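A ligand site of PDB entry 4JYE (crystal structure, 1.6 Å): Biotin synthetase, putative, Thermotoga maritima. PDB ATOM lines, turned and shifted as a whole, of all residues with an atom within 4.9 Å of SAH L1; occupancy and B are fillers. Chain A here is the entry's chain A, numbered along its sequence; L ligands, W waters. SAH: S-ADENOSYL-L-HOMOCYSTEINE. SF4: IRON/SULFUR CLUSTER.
Merely in contact with SAH L1: Pro 229, Leu 305, Tyr 303, Ser 136, Tyr 306, Gly 138, Gln 107, Cys 70 and Phe 230. Hydrophobic or aromatic side chains within 4 Å of SAH L1: Tyr 69, Met 199, Ile 231, Leu 305 and Tyr 306. The nearest printed residue that does not touch SAH L1 is Gly 109 (4.003 Å).
Water W1 bridges an oxygen (O3') of SAH L1 (2.7 Å) and the backbone NH (N) of Arg 159 (3.0 Å). Water W5 lies within hydrogen-bond range of O of Leu 157 (2.7 Å), OXT of SAH L1 (2.8 Å), N of Gly 138 (3.0 Å), OG of Ser 136 (3.1 Å) and N of Leu 137 (3.3 Å). Water W6 lies within hydrogen-bond range of NH1 of Arg 159 (2.9 Å) and N3 of SAH L1 (2.9 Å). Water W4 lies within hydrogen-bond range of the side-chain carboxylate (OE2) of Glu 110 (2.7 Å), the guanidinium group (NH1) of Arg 180 (2.8 Å), a sulfur (S4) of SF4 L2 (3.3 Å) and the guanidinium group (NH2) of Arg 172 (3.3 Å). Water W2 lies within hydrogen-bond range of the side-chain carboxylate of Glu 161 (2.6 Å), the side-chain hydroxyl of Tyr 69 (2.8 Å), the guanidinium group of Arg 172 (3.2 Å) and a sulfur (S3) of SF4 L2 (3.3 Å).
The side-chain hydroxyl (OH) of Tyr 306 is in hydrogen-bond range of the backbone NH (N) of Ala 270. O of Ser 136 sits at hydrogen-bond distance from N of Ser 108, at 3.3 Å. O of Leu 157 is in hydrogen-bond range of OG of Ser 136, 3.4 Å away. The side-chain hydroxyl of Ser 136 lies within hydrogen-bond range of the side-chain amide nitrogen of Gln 107, at 3.1 Å. NE of Arg 180 lies within hydrogen-bond range of O of Arg 159 (2.7 Å). The side-chain hydroxyl (OH) of Tyr 303 lies within hydrogen-bond range of the side-chain amide oxygen (OE1) of Gln 107. The guanidinium group (NH2) of Arg 180 is in salt-bridge range of the side-chain carboxylate (OE2) of Glu 161. N of Met 199 is in hydrogen-bond range of O of Glu 161 (3.3 Å).
O of SAH L1 is bound to FE2 of SF4 L2 (2.3 Å).
N1 of SAH L1 sits at hydrogen-bond distance from N of Ile 231 (3.1 Å). O of Tyr 69 sits at hydrogen-bond distance from N6 of SAH L1, at 2.8 Å. OE2 of Glu 161 sits at hydrogen-bond distance from O3' of SAH L1 (2.6 Å). The side-chain sulfur (SG) of Cys 70 is bound to an iron atom (FE4) of SF4 L2, at 2.2 Å. The side-chain sulfur of Met 199 sits close to an oxygen (O2') of SAH L1 (3.8 Å). A nitrogen (N) of SAH L1 sits close to the backbone carbonyl oxygen (O) of Ser 108 (3.1 Å). O of Ile 231 lies within hydrogen-bond range of N6 of SAH L1 (2.8 Å). The guanidinium group (NH1) of Arg 159 is in hydrogen-bond range of an oxygen (O2') of SAH L1 (3.0 Å). NH2 of Arg 180 lies within salt-bridge range of OXT of SAH L1.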
ATOM      1  N   TYR A  69     -18.952  15.585  -4.191  1.00  0.00           N
ATOM      2  CA  TYR A  69     -19.932  16.366  -4.932  1.00  0.00           C
ATOM      3  C   TYR A  69     -21.102  15.579  -5.466  1.00  0.00           C
ATOM      4  O   TYR A  69     -22.102  16.197  -5.922  1.00  0.00           O
ATOM      5  CB  TYR A  69     -19.234  17.042  -6.151  1.00  0.00           C
ATOM      6  CG  TYR A  69     -18.331  16.138  -6.946  1.00  0.00           C
ATOM      7  CD1 TYR A  69     -18.842  15.215  -7.871  1.00  0.00           C
ATOM      8  CD2 TYR A  69     -16.950  16.172  -6.776  1.00  0.00           C
ATOM      9  CE1 TYR A  69     -17.983  14.396  -8.612  1.00  0.00           C
ATOM     10  CE2 TYR A  69     -16.108  15.354  -7.483  1.00  0.00           C
ATOM     11  CZ  TYR A  69     -16.621  14.476  -8.407  1.00  0.00           C
ATOM     12  OH  TYR A  69     -15.761  13.659  -9.101  1.00  0.00           O
ATOM     13  N   CYS A  70     -21.023  14.244  -5.405  1.00  0.00           N
ATOM     14  CA  CYS A  70     -21.923  13.374  -6.184  1.00  0.00           C
ATOM     15  C   CYS A  70     -23.019  12.730  -5.363  1.00  0.00           C
ATOM     16  O   CYS A  70     -22.729  12.055  -4.358  1.00  0.00           O
ATOM     17  CB  CYS A  70     -21.117  12.274  -6.849  1.00  0.00           C
ATOM     18  SG  CYS A  70     -22.054  11.310  -8.029  1.00  0.00           S
ATOM     19  N   GLN A 107     -23.589   4.633 -19.204  1.00  0.00           N
ATOM     20  CA  GLN A 107     -23.012   5.308 -18.044  1.00  0.00           C
ATOM     21  C   GLN A 107     -23.550   4.695 -16.763  1.00  0.00           C
ATOM     22  O   GLN A 107     -24.707   4.289 -16.689  1.00  0.00           O
ATOM     23  CB  GLN A 107     -23.292   6.816 -18.080  1.00  0.00           C
ATOM     24  CG  GLN A 107     -22.533   7.582 -17.012  1.00  0.00           C
ATOM     25  CD  GLN A 107     -22.738   9.082 -17.093  1.00  0.00           C
ATOM     26  OE1 GLN A 107     -23.722   9.618 -16.563  1.00  0.00           O
ATOM     27  NE2 GLN A 107     -21.803   9.768 -17.742  1.00  0.00           N
ATOM     28  N   SER A 108     -22.699   4.655 -15.740  1.00  0.00           N
ATOM     29  CA  SER A 108     -23.102   4.176 -14.415  1.00  0.00           C
ATOM     30  C   SER A 108     -22.219   4.739 -13.323  1.00  0.00           C
ATOM     31  O   SER A 108     -21.165   5.370 -13.567  1.00  0.00           O
ATOM     32  CB  SER A 108     -23.035   2.638 -14.383  1.00  0.00           C
ATOM     33  OG  SER A 108     -21.694   2.203 -14.550  1.00  0.00           O
ATOM     34  N   GLY A 109     -22.655   4.515 -12.082  1.00  0.00           N
ATOM     35  CA  GLY A 109     -21.726   4.590 -10.972  1.00  0.00           C
ATOM     36  C   GLY A 109     -20.680   3.509 -11.153  1.00  0.00           C
ATOM     37  O   GLY A 109     -20.799   2.619 -12.020  1.00  0.00           O
ATOM     38  N   GLU A 110     -19.623   3.569 -10.362  1.00  0.00           N
ATOM     39  CA  GLU A 110     -18.655   2.489 -10.297  1.00  0.00           C
ATOM     40  C   GLU A 110     -19.233   1.293  -9.571  1.00  0.00           C
ATOM     41  O   GLU A 110     -18.991   1.071  -8.354  1.00  0.00           O
ATOM     42  CB  GLU A 110     -17.334   2.933  -9.676  1.00  0.00           C
ATOM     43  CG  GLU A 110     -16.570   3.964 -10.525  1.00  0.00           C
ATOM     44  CD  GLU A 110     -15.096   4.123 -10.138  1.00  0.00           C
ATOM     45  OE1 GLU A 110     -14.600   3.374  -9.277  1.00  0.00           O
ATOM     46  OE2 GLU A 110     -14.436   5.018 -10.746  1.00  0.00           O
ATOM     47  N   SER A 136     -18.939   5.041 -20.091  1.00  0.00           N
ATOM     48  CA  SER A 136     -18.643   6.013 -19.048  1.00  0.00           C
ATOM     49  C   SER A 136     -18.864   5.353 -17.698  1.00  0.00           C
ATOM     50  O   SER A 136     -19.850   5.603 -17.024  1.00  0.00           O
ATOM     51  CB  SER A 136     -19.501   7.289 -19.254  1.00  0.00           C
ATOM     52  OG  SER A 136     -19.168   8.326 -18.334  1.00  0.00           O
ATOM     53  N   LEU A 137     -17.890   4.542 -17.276  1.00  0.00           N
ATOM     54  CA  LEU A 137     -18.020   3.654 -16.132  1.00  0.00           C
ATOM     55  C   LEU A 137     -17.062   3.946 -14.987  1.00  0.00           C
ATOM     56  O   LEU A 137     -17.056   3.190 -13.981  1.00  0.00           O
ATOM     57  CB  LEU A 137     -17.816   2.198 -16.558  1.00  0.00           C
ATOM     58  CG  LEU A 137     -18.604   1.724 -17.780  1.00  0.00           C
ATOM     59  CD1 LEU A 137     -18.323   0.253 -18.143  1.00  0.00           C
ATOM     60  CD2 LEU A 137     -20.119   2.024 -17.612  1.00  0.00           C
ATOM     61  N   GLY A 138     -16.241   4.997 -15.110  1.00  0.00           N
ATOM     62  CA  GLY A 138     -15.265   5.315 -14.097  1.00  0.00           C
ATOM     63  C   GLY A 138     -13.892   4.675 -14.303  1.00  0.00           C
ATOM     64  O   GLY A 138     -13.494   4.339 -15.422  1.00  0.00           O
ATOM     65  N   LEU A 157     -15.709   8.129 -21.919  1.00  0.00           N
ATOM     66  CA  LEU A 157     -15.804   9.418 -21.270  1.00  0.00           C
ATOM     67  C   LEU A 157     -15.318   9.270 -19.834  1.00  0.00           C
ATOM     68  O   LEU A 157     -15.886   8.499 -19.055  1.00  0.00           O
ATOM     69  CB  LEU A 157     -17.240   9.946 -21.239  1.00  0.00           C
ATOM     70  CG  LEU A 157     -18.030   9.870 -22.524  1.00  0.00           C
ATOM     71  CD1 LEU A 157     -19.497  10.414 -22.407  1.00  0.00           C
ATOM     72  CD2 LEU A 157     -17.238  10.572 -23.611  1.00  0.00           C
ATOM     73  N   LEU A 158     -14.307  10.035 -19.489  1.00  0.00           N
ATOM     74  CA  LEU A 158     -13.761  10.032 -18.133  1.00  0.00           C
ATOM     75  C   LEU A 158     -13.276  11.432 -17.817  1.00  0.00           C
ATOM     76  O   LEU A 158     -12.100  11.777 -18.013  1.00  0.00           O
ATOM     77  CB  LEU A 158     -12.641   8.993 -18.039  1.00  0.00           C
ATOM     78  CG  LEU A 158     -12.216   8.648 -16.608  1.00  0.00           C
ATOM     79  CD1 LEU A 158     -13.224   7.785 -15.874  1.00  0.00           C
ATOM     80  CD2 LEU A 158     -10.853   7.956 -16.626  1.00  0.00           C
ATOM     81  N   ARG A 159     -14.203  12.280 -17.370  1.00  0.00           N
ATOM     82  CA  ARG A 159     -13.844  13.669 -17.100  1.00  0.00           C
ATOM     83  C   ARG A 159     -12.723  13.707 -16.058  1.00  0.00           C
ATOM     84  O   ARG A 159     -12.738  12.940 -15.093  1.00  0.00           O
ATOM     85  CB  ARG A 159     -15.046  14.410 -16.551  1.00  0.00           C
ATOM     86  CG  ARG A 159     -16.154  14.598 -17.542  1.00  0.00           C
ATOM     87  CD  ARG A 159     -17.182  15.462 -16.921  1.00  0.00           C
ATOM     88  NE  ARG A 159     -18.382  15.604 -17.748  1.00  0.00           N
ATOM     89  CZ  ARG A 159     -19.452  16.296 -17.378  1.00  0.00           C
ATOM     90  NH1 ARG A 159     -19.490  16.874 -16.172  1.00  0.00           N
ATOM     91  NH2 ARG A 159     -20.502  16.386 -18.203  1.00  0.00           N
ATOM     92  N   GLU A 161     -12.213  16.199 -14.107  1.00  0.00           N
ATOM     93  CA  GLU A 161     -12.910  16.797 -12.955  1.00  0.00           C
ATOM     94  C   GLU A 161     -12.267  18.108 -12.510  1.00  0.00           C
ATOM     95  O   GLU A 161     -12.912  19.165 -12.527  1.00  0.00           O
ATOM     96  CB  GLU A 161     -13.019  15.832 -11.759  1.00  0.00           C
ATOM     97  CG  GLU A 161     -13.587  14.418 -12.063  1.00  0.00           C
ATOM     98  CD  GLU A 161     -14.970  14.392 -12.738  1.00  0.00           C
ATOM     99  OE1 GLU A 161     -15.585  15.463 -13.040  1.00  0.00           O
ATOM    100  OE2 GLU A 161     -15.423  13.247 -12.975  1.00  0.00           O
ATOM    101  N   ARG A 172     -12.214  13.693  -4.098  1.00  0.00           N
ATOM    102  CA  ARG A 172     -12.359  12.341  -4.610  1.00  0.00           C
ATOM    103  C   ARG A 172     -11.431  11.458  -3.777  1.00  0.00           C
ATOM    104  O   ARG A 172     -10.371  11.026  -4.249  1.00  0.00           O
ATOM    105  CB  ARG A 172     -12.033  12.305  -6.117  1.00  0.00           C
ATOM    106  CG  ARG A 172     -12.822  13.351  -6.915  1.00  0.00           C
ATOM    107  CD  ARG A 172     -12.716  13.145  -8.408  1.00  0.00           C
ATOM    108  NE  ARG A 172     -13.374  11.892  -8.745  1.00  0.00           N
ATOM    109  CZ  ARG A 172     -12.786  10.813  -9.238  1.00  0.00           C
ATOM    110  NH1 ARG A 172     -11.498  10.815  -9.586  1.00  0.00           N
ATOM    111  NH2 ARG A 172     -13.506   9.712  -9.408  1.00  0.00           N
ATOM    112  N   ARG A 180      -6.510   9.292 -12.261  1.00  0.00           N
ATOM    113  CA  ARG A 180      -7.419   9.742 -13.343  1.00  0.00           C
ATOM    114  C   ARG A 180      -6.690   9.915 -14.665  1.00  0.00           C
ATOM    115  O   ARG A 180      -7.146   9.455 -15.718  1.00  0.00           O
ATOM    116  CB  ARG A 180      -8.107  11.062 -12.953  1.00  0.00           C
ATOM    117  CG  ARG A 180      -9.440  11.308 -13.619  1.00  0.00           C
ATOM    118  CD  ARG A 180     -10.541  10.413 -13.075  1.00  0.00           C
ATOM    119  NE  ARG A 180     -11.843  10.837 -13.601  1.00  0.00           N
ATOM    120  CZ  ARG A 180     -12.997  10.207 -13.385  1.00  0.00           C
ATOM    121  NH1 ARG A 180     -13.037   9.130 -12.618  1.00  0.00           N
ATOM    122  NH2 ARG A 180     -14.139  10.674 -13.926  1.00  0.00           N
ATOM    123  N   MET A 199     -15.698  20.065 -13.978  1.00  0.00           N
ATOM    124  CA  MET A 199     -16.759  20.896 -13.409  1.00  0.00           C
ATOM    125  C   MET A 199     -16.204  22.297 -13.136  1.00  0.00           C
ATOM    126  O   MET A 199     -15.002  22.477 -12.896  1.00  0.00           O
ATOM    127  CB  MET A 199     -17.354  20.296 -12.124  1.00  0.00           C
ATOM    128  CG  MET A 199     -18.187  19.029 -12.351  1.00  0.00           C
ATOM    129  SD  MET A 199     -18.659  18.168 -10.835  1.00  0.00           S
ATOM    130  CE  MET A 199     -17.085  17.456 -10.380  1.00  0.00           C
ATOM    131  N   PRO A 229     -21.421  23.014 -14.950  1.00  0.00           N
ATOM    132  CA  PRO A 229     -21.318  23.674 -13.662  1.00  0.00           C
ATOM    133  C   PRO A 229     -21.460  22.675 -12.519  1.00  0.00           C
ATOM    134  O   PRO A 229     -22.234  21.723 -12.624  1.00  0.00           O
ATOM    135  CB  PRO A 229     -22.504  24.649 -13.701  1.00  0.00           C
ATOM    136  CG  PRO A 229     -23.544  23.872 -14.438  1.00  0.00           C
ATOM    137  CD  PRO A 229     -22.774  23.137 -15.501  1.00  0.00           C
ATOM    138  N   PHE A 230     -20.721  22.880 -11.430  1.00  0.00           N
ATOM    139  CA  PHE A 230     -21.040  22.191 -10.189  1.00  0.00           C
ATOM    140  C   PHE A 230     -22.437  22.565  -9.638  1.00  0.00           C
ATOM    141  O   PHE A 230     -22.781  23.752  -9.483  1.00  0.00           O
ATOM    142  CB  PHE A 230     -19.965  22.467  -9.137  1.00  0.00           C
ATOM    143  CG  PHE A 230     -20.382  22.097  -7.734  1.00  0.00           C
ATOM    144  CD1 PHE A 230     -20.543  20.774  -7.361  1.00  0.00           C
ATOM    145  CD2 PHE A 230     -20.596  23.070  -6.782  1.00  0.00           C
ATOM    146  CE1 PHE A 230     -20.959  20.431  -6.057  1.00  0.00           C
ATOM    147  CE2 PHE A 230     -20.970  22.733  -5.484  1.00  0.00           C
ATOM    148  CZ  PHE A 230     -21.159  21.412  -5.134  1.00  0.00           C
ATOM    149  N   ILE A 231     -23.225  21.548  -9.348  1.00  0.00           N
ATOM    150  CA  ILE A 231     -24.569  21.699  -8.810  1.00  0.00           C
ATOM    151  C   ILE A 231     -24.660  20.949  -7.467  1.00  0.00           C
ATOM    152  O   ILE A 231     -24.643  19.716  -7.446  1.00  0.00           O
ATOM    153  CB  ILE A 231     -25.691  21.175  -9.757  1.00  0.00           C
ATOM    154  CG1 ILE A 231     -25.639  21.887 -11.122  1.00  0.00           C
ATOM    155  CG2 ILE A 231     -27.105  21.383  -9.101  1.00  0.00           C
ATOM    156  CD1 ILE A 231     -26.562  21.300 -12.194  1.00  0.00           C
ATOM    157  N   PRO A 232     -24.733  21.698  -6.321  1.00  0.00           N
ATOM    158  CA  PRO A 232     -24.725  21.011  -5.031  1.00  0.00           C
ATOM    159  C   PRO A 232     -25.917  20.087  -4.800  1.00  0.00           C
ATOM    160  O   PRO A 232     -27.041  20.376  -5.186  1.00  0.00           O
ATOM    161  CB  PRO A 232     -24.715  22.170  -4.027  1.00  0.00           C
ATOM    162  CG  PRO A 232     -25.453  23.263  -4.719  1.00  0.00           C
ATOM    163  CD  PRO A 232     -25.134  23.115  -6.195  1.00  0.00           C
ATOM    164  N   ALA A 270     -26.272  19.271 -17.268  1.00  0.00           N
ATOM    165  CA  ALA A 270     -26.090  20.228 -16.159  1.00  0.00           C
ATOM    166  C   ALA A 270     -26.283  21.680 -16.626  1.00  0.00           C
ATOM    167  O   ALA A 270     -26.876  22.492 -15.889  1.00  0.00           O
ATOM    168  CB  ALA A 270     -24.707  20.023 -15.424  1.00  0.00           C
ATOM    169  N   TYR A 303     -31.247   8.453 -10.903  1.00  0.00           N
ATOM    170  CA  TYR A 303     -29.877   8.719 -11.289  1.00  0.00           C
ATOM    171  C   TYR A 303     -29.540  10.162 -10.981  1.00  0.00           C
ATOM    172  O   TYR A 303     -29.479  11.012 -11.866  1.00  0.00           O
ATOM    173  CB  TYR A 303     -29.614   8.337 -12.743  1.00  0.00           C
ATOM    174  CG  TYR A 303     -28.151   8.244 -13.099  1.00  0.00           C
ATOM    175  CD1 TYR A 303     -27.414   7.113 -12.800  1.00  0.00           C
ATOM    176  CD2 TYR A 303     -27.521   9.264 -13.790  1.00  0.00           C
ATOM    177  CE1 TYR A 303     -26.069   7.010 -13.132  1.00  0.00           C
ATOM    178  CE2 TYR A 303     -26.188   9.177 -14.137  1.00  0.00           C
ATOM    179  CZ  TYR A 303     -25.475   8.057 -13.833  1.00  0.00           C
ATOM    180  OH  TYR A 303     -24.144   8.030 -14.205  1.00  0.00           O
ATOM    181  N   LEU A 305     -26.976  12.405  -9.836  1.00  0.00           N
ATOM    182  CA  LEU A 305     -25.657  12.993  -9.638  1.00  0.00           C
ATOM    183  C   LEU A 305     -25.813  14.349  -8.934  1.00  0.00           C
ATOM    184  O   LEU A 305     -25.071  14.663  -8.013  1.00  0.00           O
ATOM    185  CB  LEU A 305     -24.945  13.179 -11.000  1.00  0.00           C
ATOM    186  CG  LEU A 305     -24.788  11.923 -11.854  1.00  0.00           C
ATOM    187  CD1 LEU A 305     -24.191  12.343 -13.223  1.00  0.00           C
ATOM    188  CD2 LEU A 305     -23.909  10.872 -11.190  1.00  0.00           C
ATOM    189  N   TYR A 306     -26.766  15.141  -9.443  1.00  0.00           N
ATOM    190  CA  TYR A 306     -27.167  16.438  -8.917  1.00  0.00           C
ATOM    191  C   TYR A 306     -28.667  16.489  -8.969  1.00  0.00           C
ATOM    192  O   TYR A 306     -29.276  15.767  -9.782  1.00  0.00           O
ATOM    193  CB  TYR A 306     -26.532  17.573  -9.739  1.00  0.00           C
ATOM    194  CG  TYR A 306     -26.644  17.391 -11.230  1.00  0.00           C
ATOM    195  CD1 TYR A 306     -27.799  17.770 -11.909  1.00  0.00           C
ATOM    196  CD2 TYR A 306     -25.608  16.848 -11.965  1.00  0.00           C
ATOM    197  CE1 TYR A 306     -27.931  17.607 -13.266  1.00  0.00           C
ATOM    198  CE2 TYR A 306     -25.714  16.687 -13.353  1.00  0.00           C
ATOM    199  CZ  TYR A 306     -26.896  17.054 -13.983  1.00  0.00           C
ATOM    200  OH  TYR A 306     -27.066  16.904 -15.323  1.00  0.00           O
HETATM  201  N   SAH L   1     -19.022   7.222 -12.307  1.00  0.00           N
HETATM  202  CA  SAH L   1     -18.464   7.734 -13.607  1.00  0.00           C
HETATM  203  CB  SAH L   1     -19.629   8.246 -14.487  1.00  0.00           C
HETATM  204  CG  SAH L   1     -20.777   8.907 -13.717  1.00  0.00           C
HETATM  205  SD  SAH L   1     -20.384  10.528 -13.065  1.00  0.00           S
HETATM  206  C   SAH L   1     -17.459   8.816 -13.355  1.00  0.00           C
HETATM  207  O   SAH L   1     -17.294   9.305 -12.199  1.00  0.00           O
HETATM  208  OXT SAH L   1     -16.767   9.178 -14.310  1.00  0.00           O
HETATM  209  C5' SAH L   1     -20.478  11.533 -14.531  1.00  0.00           C
HETATM  210  C4' SAH L   1     -20.053  13.008 -14.337  1.00  0.00           C
HETATM  211  O4' SAH L   1     -21.058  13.699 -13.591  1.00  0.00           O
HETATM  212  C3' SAH L   1     -18.793  13.280 -13.539  1.00  0.00           C
HETATM  213  O3' SAH L   1     -17.594  13.087 -14.309  1.00  0.00           O
HETATM  214  C2' SAH L   1     -19.009  14.692 -12.989  1.00  0.00           C
HETATM  215  O2' SAH L   1     -18.270  15.714 -13.697  1.00  0.00           O
HETATM  216  C1' SAH L   1     -20.519  14.911 -13.123  1.00  0.00           C
HETATM  217  N9  SAH L   1     -21.103  15.264 -11.823  1.00  0.00           N
HETATM  218  C8  SAH L   1     -21.145  14.464 -10.719  1.00  0.00           C
HETATM  219  N7  SAH L   1     -21.685  15.131  -9.659  1.00  0.00           N
HETATM  220  C5  SAH L   1     -22.010  16.372 -10.131  1.00  0.00           C
HETATM  221  C6  SAH L   1     -22.627  17.574  -9.551  1.00  0.00           C
HETATM  222  N6  SAH L   1     -23.010  17.569  -8.238  1.00  0.00           N
HETATM  223  N1  SAH L   1     -22.750  18.685 -10.342  1.00  0.00           N
HETATM  224  C2  SAH L   1     -22.405  18.676 -11.653  1.00  0.00           C
HETATM  225  N3  SAH L   1     -21.842  17.603 -12.247  1.00  0.00           N
HETATM  226  C4  SAH L   1     -21.612  16.469 -11.543  1.00  0.00           C
HETATM  227 FE1  SF4 L   2     -17.801   9.591  -8.083  1.00  0.00          FE
HETATM  228 FE2  SF4 L   2     -18.821   8.793 -10.627  1.00  0.00          FE
HETATM  229 FE3  SF4 L   2     -19.418   7.404  -8.184  1.00  0.00          FE
HETATM  230 FE4  SF4 L   2     -20.437   9.861  -8.580  1.00  0.00          FE
HETATM  231  S1  SF4 L   2     -20.879   8.044  -9.858  1.00  0.00           S
HETATM  232  S2  SF4 L   2     -19.498   9.055  -6.633  1.00  0.00           S
HETATM  233  S3  SF4 L   2     -18.763  10.937  -9.737  1.00  0.00           S
HETATM  234  S4  SF4 L   2     -17.365   7.648  -9.195  1.00  0.00           S
HETATM  235  O   HOH W   1     -16.825  11.295 -16.174  1.00  0.00           O
HETATM  236  O   HOH W   2     -15.749  11.606 -10.934  1.00  0.00           O
HETATM  237  O   HOH W   3     -22.675  14.024 -15.991  1.00  0.00           O
HETATM  238  O   HOH W   4     -14.986   7.562 -11.460  1.00  0.00           O
HETATM  239  O   HOH W   5     -16.664   7.566 -16.596  1.00  0.00           O
HETATM  240  O   HOH W   6     -21.591  18.436 -15.008  1.00  0.00           O
